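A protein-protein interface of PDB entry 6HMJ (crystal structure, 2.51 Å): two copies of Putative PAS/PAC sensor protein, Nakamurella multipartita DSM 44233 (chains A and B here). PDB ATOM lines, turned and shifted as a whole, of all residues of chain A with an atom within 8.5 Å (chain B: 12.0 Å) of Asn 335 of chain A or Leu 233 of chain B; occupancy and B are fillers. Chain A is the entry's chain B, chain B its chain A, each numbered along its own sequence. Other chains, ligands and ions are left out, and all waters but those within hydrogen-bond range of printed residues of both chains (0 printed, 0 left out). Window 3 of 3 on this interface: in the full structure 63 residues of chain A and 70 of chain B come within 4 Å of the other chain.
OD1 of Asn 335 of chain A lies close to N of Ala 337 of chain A.
OD1 of Asn 335 of chain A lies within hydrogen-bond range of N of Gly 338 of chain A (3.0 Å).
The backbone carbonyl oxygen of His 342 of chain A lies within hydrogen-bond range of the backbone NH of Val 333 of chain A.
The side-chain amide oxygen (OD1) of Asn 335 of chain A lies within hydrogen-bond range of the backbone NH (N) of Arg 339 of chain A (2.7 Å).
The backbone NH of Thr 341 of chain A lies within hydrogen-bond range of the backbone carbonyl oxygen of Val 333 of chain A.
The backbone carbonyl oxygen of Pro 235 of chain B lies within hydrogen-bond range of the side-chain hydroxyl of Thr 239 of chain B (2.6 Å).
Pro 235 of chain B touches Leu 238 of chain A.
Leu 238 of chain A touches Leu 238 of chain B.
Leu 238 of chain A touches Thr 239 of chain B (CD1 to OG1, 2.9 Å).
Val 251 of chain A touches Ile 237 of chain B.
CD2 of Leu 233 of chain B touches CB of Asn 335 of chain A, at 3.97 Å.
CD of Pro 230 of chain B touches NE2 of His 342 of chain A, at 3.8 Å.
CE1 of His 342 of chain A touches CD1 of Leu 233 of chain B, at 3.7 Å.
O of Ile 237 of chain B touches CD1 of Ile 344 of chain A, 3.2 Å away.
CG of Arg 240 of chain B touches CD1 of Ile 344 of chain A, 3.5 Å away.
Ile 344 of chain A touches Ala 241 of chain B (CD1 to N, 3.8 Å).
Val 333 of chain A touches one residue of chain B.
Of chain B, only Leu 233 (3.97 Å) comes within 4 Å of Asn 335 of chain A.
No residue of chain B comes within 4 Å of Gly 336 of chain A.
Arg 339 of chain A touches none of the printed residues of chain B.
Val 340 of chain A touches none of the printed residues of chain B.
Of the printed residues of chain A, Pro 230 of chain B touches His 342.
No residue of chain A comes within 4 Å of Ala 232 of chain B.
Of the printed residues of chain A, Leu 238 of chain B touches Leu 238 (3.8 Å).
The nearest residue of chain B that does not touch Asn 335 of chain A is Gly 236 of chain B (7.8 Å).
The nearest printed residue of chain A that does not touch Leu 233 of chain B is Gly 336 of chain A (5.3 Å).
The nearest printed residue of chain A that does not touch Leu 238 of chain B is Val 251 of chain A (5.2 Å).
Of the 16 printed residues of chain A, 7 touch a printed residue of chain B.
Hydrophobic or aromatic side chains of chain A that line the printed part of chain B: Leu 238, Val 251, Val 333, His 342 and Ile 344.
Along chain B the printed residues that touch a printed residue of chain A span positions 230 to 241.
Among the printed residues, 13 pairs touch across the chains.
Among the printed residues, no Asp or Glu carboxylate lies within 4 Å of a Lys or Arg side-chain nitrogen of the other chain.
Leu 238 of chain B touches its own counterpart, Leu 238 of chain A.
1 position is printed for both chains.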
ATOM      1  N   LEU A 238       1.576   4.879 -27.443  1.00  0.00           N
ATOM      2  CA  LEU A 238       2.813   5.595 -27.723  1.00  0.00           C
ATOM      3  C   LEU A 238       4.029   4.687 -27.604  1.00  0.00           C
ATOM      4  O   LEU A 238       5.008   4.864 -28.336  1.00  0.00           O
ATOM      5  CB  LEU A 238       2.946   6.777 -26.760  1.00  0.00           C
ATOM      6  CG  LEU A 238       1.990   7.956 -26.952  1.00  0.00           C
ATOM      7  CD1 LEU A 238       2.372   9.092 -26.027  1.00  0.00           C
ATOM      8  CD2 LEU A 238       1.991   8.438 -28.394  1.00  0.00           C
ATOM      9  N   VAL A 251      16.385   7.731 -26.145  1.00  0.00           N
ATOM     10  CA  VAL A 251      16.127   8.592 -25.000  1.00  0.00           C
ATOM     11  C   VAL A 251      17.315   8.482 -24.057  1.00  0.00           C
ATOM     12  O   VAL A 251      17.783   7.375 -23.767  1.00  0.00           O
ATOM     13  CB  VAL A 251      14.822   8.217 -24.272  1.00  0.00           C
ATOM     14  CG1 VAL A 251      14.573   9.155 -23.095  1.00  0.00           C
ATOM     15  CG2 VAL A 251      13.646   8.248 -25.235  1.00  0.00           C
ATOM     16  N   ASP A 253      18.869   9.882 -20.239  1.00  0.00           N
ATOM     17  CA  ASP A 253      18.572  10.496 -18.948  1.00  0.00           C
ATOM     18  C   ASP A 253      19.692  11.482 -18.646  1.00  0.00           C
ATOM     19  O   ASP A 253      20.760  11.099 -18.162  1.00  0.00           O
ATOM     20  CB  ASP A 253      18.445   9.433 -17.864  1.00  0.00           C
ATOM     21  CG  ASP A 253      18.225  10.024 -16.480  1.00  0.00           C
ATOM     22  OD1 ASP A 253      17.924  11.233 -16.371  1.00  0.00           O
ATOM     23  OD2 ASP A 253      18.367   9.274 -15.493  1.00  0.00           O
ATOM     24  N   THR A 255      19.883  13.572 -16.407  1.00  0.00           N
ATOM     25  CA  THR A 255      20.065  13.765 -14.974  1.00  0.00           C
ATOM     26  C   THR A 255      21.023  12.757 -14.355  1.00  0.00           C
ATOM     27  O   THR A 255      21.475  12.972 -13.225  1.00  0.00           O
ATOM     28  CB  THR A 255      18.718  13.672 -14.243  1.00  0.00           C
ATOM     29  OG1 THR A 255      18.311  12.299 -14.173  1.00  0.00           O
ATOM     30  CG2 THR A 255      17.643  14.501 -14.948  1.00  0.00           C
ATOM     31  N   PRO A 332      14.750  18.562 -26.203  1.00  0.00           N
ATOM     32  CA  PRO A 332      14.634  18.515 -24.743  1.00  0.00           C
ATOM     33  C   PRO A 332      13.198  18.252 -24.323  1.00  0.00           C
ATOM     34  O   PRO A 332      12.243  18.636 -25.003  1.00  0.00           O
ATOM     35  CB  PRO A 332      15.097  19.910 -24.308  1.00  0.00           C
ATOM     36  CG  PRO A 332      14.738  20.785 -25.454  1.00  0.00           C
ATOM     37  CD  PRO A 332      14.902  19.944 -26.696  1.00  0.00           C
ATOM     38  N   VAL A 333      13.056  17.579 -23.184  1.00  0.00           N
ATOM     39  CA  VAL A 333      11.749  17.248 -22.631  1.00  0.00           C
ATOM     40  C   VAL A 333      11.691  17.742 -21.193  1.00  0.00           C
ATOM     41  O   VAL A 333      12.617  17.499 -20.411  1.00  0.00           O
ATOM     42  CB  VAL A 333      11.464  15.735 -22.693  1.00  0.00           C
ATOM     43  CG1 VAL A 333      10.109  15.422 -22.069  1.00  0.00           C
ATOM     44  CG2 VAL A 333      11.515  15.245 -24.131  1.00  0.00           C
ATOM     45  N   ARG A 334      10.606  18.426 -20.852  1.00  0.00           N
ATOM     46  CA  ARG A 334      10.386  18.934 -19.506  1.00  0.00           C
ATOM     47  C   ARG A 334       9.471  18.003 -18.725  1.00  0.00           C
ATOM     48  O   ARG A 334       8.717  17.205 -19.290  1.00  0.00           O
ATOM     49  CB  ARG A 334       9.781  20.339 -19.548  1.00  0.00           C
ATOM     50  CG  ARG A 334      10.801  21.433 -19.783  1.00  0.00           C
ATOM     51  CD  ARG A 334      10.141  22.752 -20.143  1.00  0.00           C
ATOM     52  NE  ARG A 334      11.094  23.660 -20.771  1.00  0.00           N
ATOM     53  CZ  ARG A 334      11.921  24.464 -20.108  1.00  0.00           C
ATOM     54  NH1 ARG A 334      11.921  24.484 -18.781  1.00  0.00           N
ATOM     55  NH2 ARG A 334      12.753  25.249 -20.777  1.00  0.00           N
ATOM     56  N   ASN A 335       9.554  18.116 -17.406  1.00  0.00           N
ATOM     57  CA  ASN A 335       8.669  17.416 -16.494  1.00  0.00           C
ATOM     58  C   ASN A 335       7.594  18.380 -15.994  1.00  0.00           C
ATOM     59  O   ASN A 335       7.511  19.534 -16.423  1.00  0.00           O
ATOM     60  CB  ASN A 335       9.474  16.810 -15.342  1.00  0.00           C
ATOM     61  CG  ASN A 335      10.223  17.859 -14.533  1.00  0.00           C
ATOM     62  OD1 ASN A 335      10.102  19.060 -14.783  1.00  0.00           O
ATOM     63  ND2 ASN A 335      11.009  17.406 -13.563  1.00  0.00           N
ATOM     64  N   GLY A 336       6.749  17.892 -15.083  1.00  0.00           N
ATOM     65  CA  GLY A 336       5.702  18.736 -14.536  1.00  0.00           C
ATOM     66  C   GLY A 336       6.233  20.003 -13.899  1.00  0.00           C
ATOM     67  O   GLY A 336       5.582  21.051 -13.955  1.00  0.00           O
ATOM     68  N   ALA A 337       7.415  19.931 -13.288  1.00  0.00           N
ATOM     69  CA  ALA A 337       8.032  21.084 -12.646  1.00  0.00           C
ATOM     70  C   ALA A 337       8.672  22.044 -13.638  1.00  0.00           C
ATOM     71  O   ALA A 337       9.163  23.100 -13.228  1.00  0.00           O
ATOM     72  CB  ALA A 337       9.085  20.618 -11.636  1.00  0.00           C
ATOM     73  N   GLY A 338       8.691  21.704 -14.924  1.00  0.00           N
ATOM     74  CA  GLY A 338       9.332  22.534 -15.920  1.00  0.00           C
ATOM     75  C   GLY A 338      10.826  22.345 -16.039  1.00  0.00           C
ATOM     76  O   GLY A 338      11.483  23.149 -16.712  1.00  0.00           O
ATOM     77  N   ARG A 339      11.386  21.320 -15.401  1.00  0.00           N
ATOM     78  CA  ARG A 339      12.811  21.033 -15.491  1.00  0.00           C
ATOM     79  C   ARG A 339      13.075  20.099 -16.665  1.00  0.00           C
ATOM     80  O   ARG A 339      12.377  19.094 -16.836  1.00  0.00           O
ATOM     81  CB  ARG A 339      13.317  20.408 -14.189  1.00  0.00           C
ATOM     82  CG  ARG A 339      14.820  20.158 -14.155  1.00  0.00           C
ATOM     83  CD  ARG A 339      15.187  19.015 -13.216  1.00  0.00           C
ATOM     84  NE  ARG A 339      16.635  18.835 -13.127  1.00  0.00           N
ATOM     85  CZ  ARG A 339      17.233  17.820 -12.508  1.00  0.00           C
ATOM     86  NH1 ARG A 339      16.513  16.877 -11.914  1.00  0.00           N
ATOM     87  NH2 ARG A 339      18.558  17.749 -12.485  1.00  0.00           N
ATOM     88  N   VAL A 340      14.072  20.441 -17.478  1.00  0.00           N
ATOM     89  CA  VAL A 340      14.490  19.565 -18.570  1.00  0.00           C
ATOM     90  C   VAL A 340      15.237  18.384 -17.954  1.00  0.00           C
ATOM     91  O   VAL A 340      16.334  18.546 -17.412  1.00  0.00           O
ATOM     92  CB  VAL A 340      15.354  20.310 -19.590  1.00  0.00           C
ATOM     93  CG1 VAL A 340      15.993  19.336 -20.566  1.00  0.00           C
ATOM     94  CG2 VAL A 340      14.510  21.333 -20.343  1.00  0.00           C
ATOM     95  N   THR A 341      14.640  17.193 -18.039  1.00  0.00           N
ATOM     96  CA  THR A 341      15.193  16.001 -17.415  1.00  0.00           C
ATOM     97  C   THR A 341      15.662  14.940 -18.404  1.00  0.00           C
ATOM     98  O   THR A 341      16.529  14.137 -18.049  1.00  0.00           O
ATOM     99  CB  THR A 341      14.163  15.381 -16.457  1.00  0.00           C
ATOM    100  OG1 THR A 341      13.146  14.701 -17.198  1.00  0.00           O
ATOM    101  CG2 THR A 341      13.508  16.458 -15.616  1.00  0.00           C
ATOM    102  N   HIS A 342      15.121  14.915 -19.621  1.00  0.00           N
ATOM    103  CA  HIS A 342      15.520  13.934 -20.620  1.00  0.00           C
ATOM    104  C   HIS A 342      15.636  14.598 -21.987  1.00  0.00           C
ATOM    105  O   HIS A 342      14.990  15.613 -22.264  1.00  0.00           O
ATOM    106  CB  HIS A 342      14.519  12.767 -20.713  1.00  0.00           C
ATOM    107  CG  HIS A 342      14.556  11.830 -19.544  1.00  0.00           C
ATOM    108  ND1 HIS A 342      14.054  12.161 -18.305  1.00  0.00           N
ATOM    109  CD2 HIS A 342      15.025  10.565 -19.432  1.00  0.00           C
ATOM    110  CE1 HIS A 342      14.217  11.144 -17.478  1.00  0.00           C
ATOM    111  NE2 HIS A 342      14.806  10.163 -18.137  1.00  0.00           N
ATOM    112  N   ILE A 344      15.614  13.548 -26.272  1.00  0.00           N
ATOM    113  CA  ILE A 344      15.268  12.564 -27.290  1.00  0.00           C
ATOM    114  C   ILE A 344      16.209  12.753 -28.472  1.00  0.00           C
ATOM    115  O   ILE A 344      16.491  13.886 -28.880  1.00  0.00           O
ATOM    116  CB  ILE A 344      13.797  12.695 -27.728  1.00  0.00           C
ATOM    117  CG1 ILE A 344      12.872  12.606 -26.512  1.00  0.00           C
ATOM    118  CG2 ILE A 344      13.444  11.607 -28.735  1.00  0.00           C
ATOM    119  CD1 ILE A 344      11.436  12.965 -26.811  1.00  0.00           C
ATOM    120  N   SER B 226       9.320  -0.170 -23.000  1.00  0.00           N
ATOM    121  CA  SER B 226       9.665   1.240 -22.899  1.00  0.00           C
ATOM    122  C   SER B 226      11.047   1.442 -22.294  1.00  0.00           C
ATOM    123  O   SER B 226      11.412   2.576 -21.965  1.00  0.00           O
ATOM    124  CB  SER B 226       8.616   1.988 -22.074  1.00  0.00           C
ATOM    125  OG  SER B 226       8.427   1.376 -20.811  1.00  0.00           O
ATOM    126  N   GLY B 227      11.822   0.369 -22.148  1.00  0.00           N
ATOM    127  CA  GLY B 227      13.167   0.486 -21.621  1.00  0.00           C
ATOM    128  C   GLY B 227      13.156   0.978 -20.191  1.00  0.00           C
ATOM    129  O   GLY B 227      12.356   0.537 -19.357  1.00  0.00           O
ATOM    130  N   LEU B 228      14.061   1.909 -19.899  1.00  0.00           N
ATOM    131  CA  LEU B 228      14.223   2.455 -18.562  1.00  0.00           C
ATOM    132  C   LEU B 228      13.642   3.858 -18.443  1.00  0.00           C
ATOM    133  O   LEU B 228      14.017   4.605 -17.535  1.00  0.00           O
ATOM    134  CB  LEU B 228      15.697   2.444 -18.163  1.00  0.00           C
ATOM    135  CG  LEU B 228      16.352   1.064 -18.268  1.00  0.00           C
ATOM    136  CD1 LEU B 228      17.832   1.133 -17.939  1.00  0.00           C
ATOM    137  CD2 LEU B 228      15.647   0.067 -17.361  1.00  0.00           C
ATOM    138  N   ILE B 229      12.741   4.229 -19.347  1.00  0.00           N
ATOM    139  CA  ILE B 229      12.022   5.496 -19.191  1.00  0.00           C
ATOM    140  C   ILE B 229      11.222   5.454 -17.896  1.00  0.00           C
ATOM    141  O   ILE B 229      10.504   4.465 -17.646  1.00  0.00           O
ATOM    142  CB  ILE B 229      11.093   5.745 -20.396  1.00  0.00           C
ATOM    143  CG1 ILE B 229      11.901   5.824 -21.696  1.00  0.00           C
ATOM    144  CG2 ILE B 229      10.245   6.990 -20.152  1.00  0.00           C
ATOM    145  CD1 ILE B 229      11.049   5.905 -22.947  1.00  0.00           C
ATOM    146  N   PRO B 230      11.289   6.476 -17.043  1.00  0.00           N
ATOM    147  CA  PRO B 230      10.407   6.500 -15.871  1.00  0.00           C
ATOM    148  C   PRO B 230       8.950   6.461 -16.305  1.00  0.00           C
ATOM    149  O   PRO B 230       8.508   7.270 -17.124  1.00  0.00           O
ATOM    150  CB  PRO B 230      10.763   7.822 -15.183  1.00  0.00           C
ATOM    151  CG  PRO B 230      12.118   8.170 -15.686  1.00  0.00           C
ATOM    152  CD  PRO B 230      12.185   7.645 -17.083  1.00  0.00           C
ATOM    153  N   THR B 231       8.197   5.510 -15.744  1.00  0.00           N
ATOM    154  CA  THR B 231       6.848   5.267 -16.240  1.00  0.00           C
ATOM    155  C   THR B 231       5.970   6.503 -16.102  1.00  0.00           C
ATOM    156  O   THR B 231       4.993   6.657 -16.845  1.00  0.00           O
ATOM    157  CB  THR B 231       6.213   4.086 -15.509  1.00  0.00           C
ATOM    158  OG1 THR B 231       5.850   4.484 -14.184  1.00  0.00           O
ATOM    159  CG2 THR B 231       7.181   2.911 -15.437  1.00  0.00           C
ATOM    160  N   ALA B 232       6.294   7.390 -15.159  1.00  0.00           N
ATOM    161  CA  ALA B 232       5.537   8.629 -15.019  1.00  0.00           C
ATOM    162  C   ALA B 232       5.843   9.591 -16.160  1.00  0.00           C
ATOM    163  O   ALA B 232       4.935  10.230 -16.704  1.00  0.00           O
ATOM    164  CB  ALA B 232       5.842   9.282 -13.672  1.00  0.00           C
ATOM    165  N   LEU B 233       7.118   9.719 -16.527  1.00  0.00           N
ATOM    166  CA  LEU B 233       7.530  10.605 -17.608  1.00  0.00           C
ATOM    167  C   LEU B 233       7.309  10.003 -18.990  1.00  0.00           C
ATOM    168  O   LEU B 233       7.597  10.671 -19.990  1.00  0.00           O
ATOM    169  CB  LEU B 233       9.009  10.972 -17.443  1.00  0.00           C
ATOM    170  CG  LEU B 233       9.380  11.715 -16.159  1.00  0.00           C
ATOM    171  CD1 LEU B 233      10.870  12.011 -16.129  1.00  0.00           C
ATOM    172  CD2 LEU B 233       8.577  12.998 -16.019  1.00  0.00           C
ATOM    173  N   LEU B 234       6.810   8.770 -19.075  1.00  0.00           N
ATOM    174  CA  LEU B 234       6.687   8.113 -20.375  1.00  0.00           C
ATOM    175  C   LEU B 234       5.717   8.839 -21.295  1.00  0.00           C
ATOM    176  O   LEU B 234       6.080   9.099 -22.454  1.00  0.00           O
ATOM    177  CB  LEU B 234       6.280   6.650 -20.168  1.00  0.00           C
ATOM    178  CG  LEU B 234       6.108   5.778 -21.411  1.00  0.00           C
ATOM    179  CD1 LEU B 234       6.366   4.317 -21.053  1.00  0.00           C
ATOM    180  CD2 LEU B 234       4.725   5.940 -22.033  1.00  0.00           C
ATOM    181  N   PRO B 235       4.495   9.183 -20.875  1.00  0.00           N
ATOM    182  CA  PRO B 235       3.583   9.863 -21.813  1.00  0.00           C
ATOM    183  C   PRO B 235       4.179  11.124 -22.412  1.00  0.00           C
ATOM    184  O   PRO B 235       4.115  11.321 -23.633  1.00  0.00           O
ATOM    185  CB  PRO B 235       2.351  10.161 -20.946  1.00  0.00           C
ATOM    186  CG  PRO B 235       2.416   9.172 -19.837  1.00  0.00           C
ATOM    187  CD  PRO B 235       3.873   8.979 -19.554  1.00  0.00           C
ATOM    188  N   GLY B 236       4.764  11.990 -21.581  1.00  0.00           N
ATOM    189  CA  GLY B 236       5.364  13.207 -22.100  1.00  0.00           C
ATOM    190  C   GLY B 236       6.552  12.938 -23.005  1.00  0.00           C
ATOM    191  O   GLY B 236       6.707  13.578 -24.048  1.00  0.00           O
ATOM    192  N   ILE B 237       7.411  11.993 -22.615  1.00  0.00           N
ATOM    193  CA  ILE B 237       8.596  11.690 -23.411  1.00  0.00           C
ATOM    194  C   ILE B 237       8.194  11.138 -24.773  1.00  0.00           C
ATOM    195  O   ILE B 237       8.650  11.618 -25.819  1.00  0.00           O
ATOM    196  CB  ILE B 237       9.514  10.710 -22.655  1.00  0.00           C
ATOM    197  CG1 ILE B 237      10.206  11.427 -21.490  1.00  0.00           C
ATOM    198  CG2 ILE B 237      10.537  10.095 -23.601  1.00  0.00           C
ATOM    199  CD1 ILE B 237      11.035  10.521 -20.602  1.00  0.00           C
ATOM    200  N   LEU B 238       7.321  10.131 -24.787  1.00  0.00           N
ATOM    201  CA  LEU B 238       6.977   9.484 -26.046  1.00  0.00           C
ATOM    202  C   LEU B 238       5.997  10.309 -26.873  1.00  0.00           C
ATOM    203  O   LEU B 238       6.012  10.219 -28.104  1.00  0.00           O
ATOM    204  CB  LEU B 238       6.414   8.086 -25.787  1.00  0.00           C
ATOM    205  CG  LEU B 238       7.406   7.084 -25.182  1.00  0.00           C
ATOM    206  CD1 LEU B 238       6.768   5.707 -25.055  1.00  0.00           C
ATOM    207  CD2 LEU B 238       8.690   7.002 -25.987  1.00  0.00           C
ATOM    208  N   THR B 239       5.139  11.110 -26.235  1.00  0.00           N
ATOM    209  CA  THR B 239       4.344  12.064 -27.002  1.00  0.00           C
ATOM    210  C   THR B 239       5.256  13.007 -27.776  1.00  0.00           C
ATOM    211  O   THR B 239       5.033  13.271 -28.963  1.00  0.00           O
ATOM    212  CB  THR B 239       3.415  12.857 -26.077  1.00  0.00           C
ATOM    213  OG1 THR B 239       2.451  11.976 -25.488  1.00  0.00           O
ATOM    214  CG2 THR B 239       2.682  13.949 -26.850  1.00  0.00           C
ATOM    215  N   ARG B 240       6.300  13.510 -27.117  1.00  0.00           N
ATOM    216  CA  ARG B 240       7.302  14.308 -27.811  1.00  0.00           C
ATOM    217  C   ARG B 240       7.983  13.508 -28.914  1.00  0.00           C
ATOM    218  O   ARG B 240       8.262  14.041 -29.994  1.00  0.00           O
ATOM    219  CB  ARG B 240       8.333  14.824 -26.811  1.00  0.00           C
ATOM    220  CG  ARG B 240       9.352  15.764 -27.416  1.00  0.00           C
ATOM    221  CD  ARG B 240       8.724  17.024 -27.972  1.00  0.00           C
ATOM    222  NE  ARG B 240       9.729  18.062 -28.171  1.00  0.00           N
ATOM    223  CZ  ARG B 240       9.469  19.282 -28.625  1.00  0.00           C
ATOM    224  NH1 ARG B 240       8.227  19.630 -28.933  1.00  0.00           N
ATOM    225  NH2 ARG B 240      10.456  20.157 -28.771  1.00  0.00           N
ATOM    226  N   ALA B 241       8.256  12.225 -28.663  1.00  0.00           N
ATOM    227  CA  ALA B 241       8.952  11.409 -29.652  1.00  0.00           C
ATOM    228  C   ALA B 241       8.140  11.298 -30.935  1.00  0.00           C
ATOM    229  O   ALA B 241       8.639  11.595 -32.027  1.00  0.00           O
ATOM    230  CB  ALA B 241       9.241  10.021 -29.076  1.00  0.00           C
ATOM    231  N   ALA B 242       6.881  10.874 -30.822  1.00  0.00           N
ATOM    232  CA  ALA B 242       6.032  10.766 -32.002  1.00  0.00           C
ATOM    233  C   ALA B 242       5.850  12.112 -32.691  1.00  0.00           C
ATOM    234  O   ALA B 242       5.678  12.166 -33.914  1.00  0.00           O
ATOM    235  CB  ALA B 242       4.674  10.183 -31.615  1.00  0.00           C
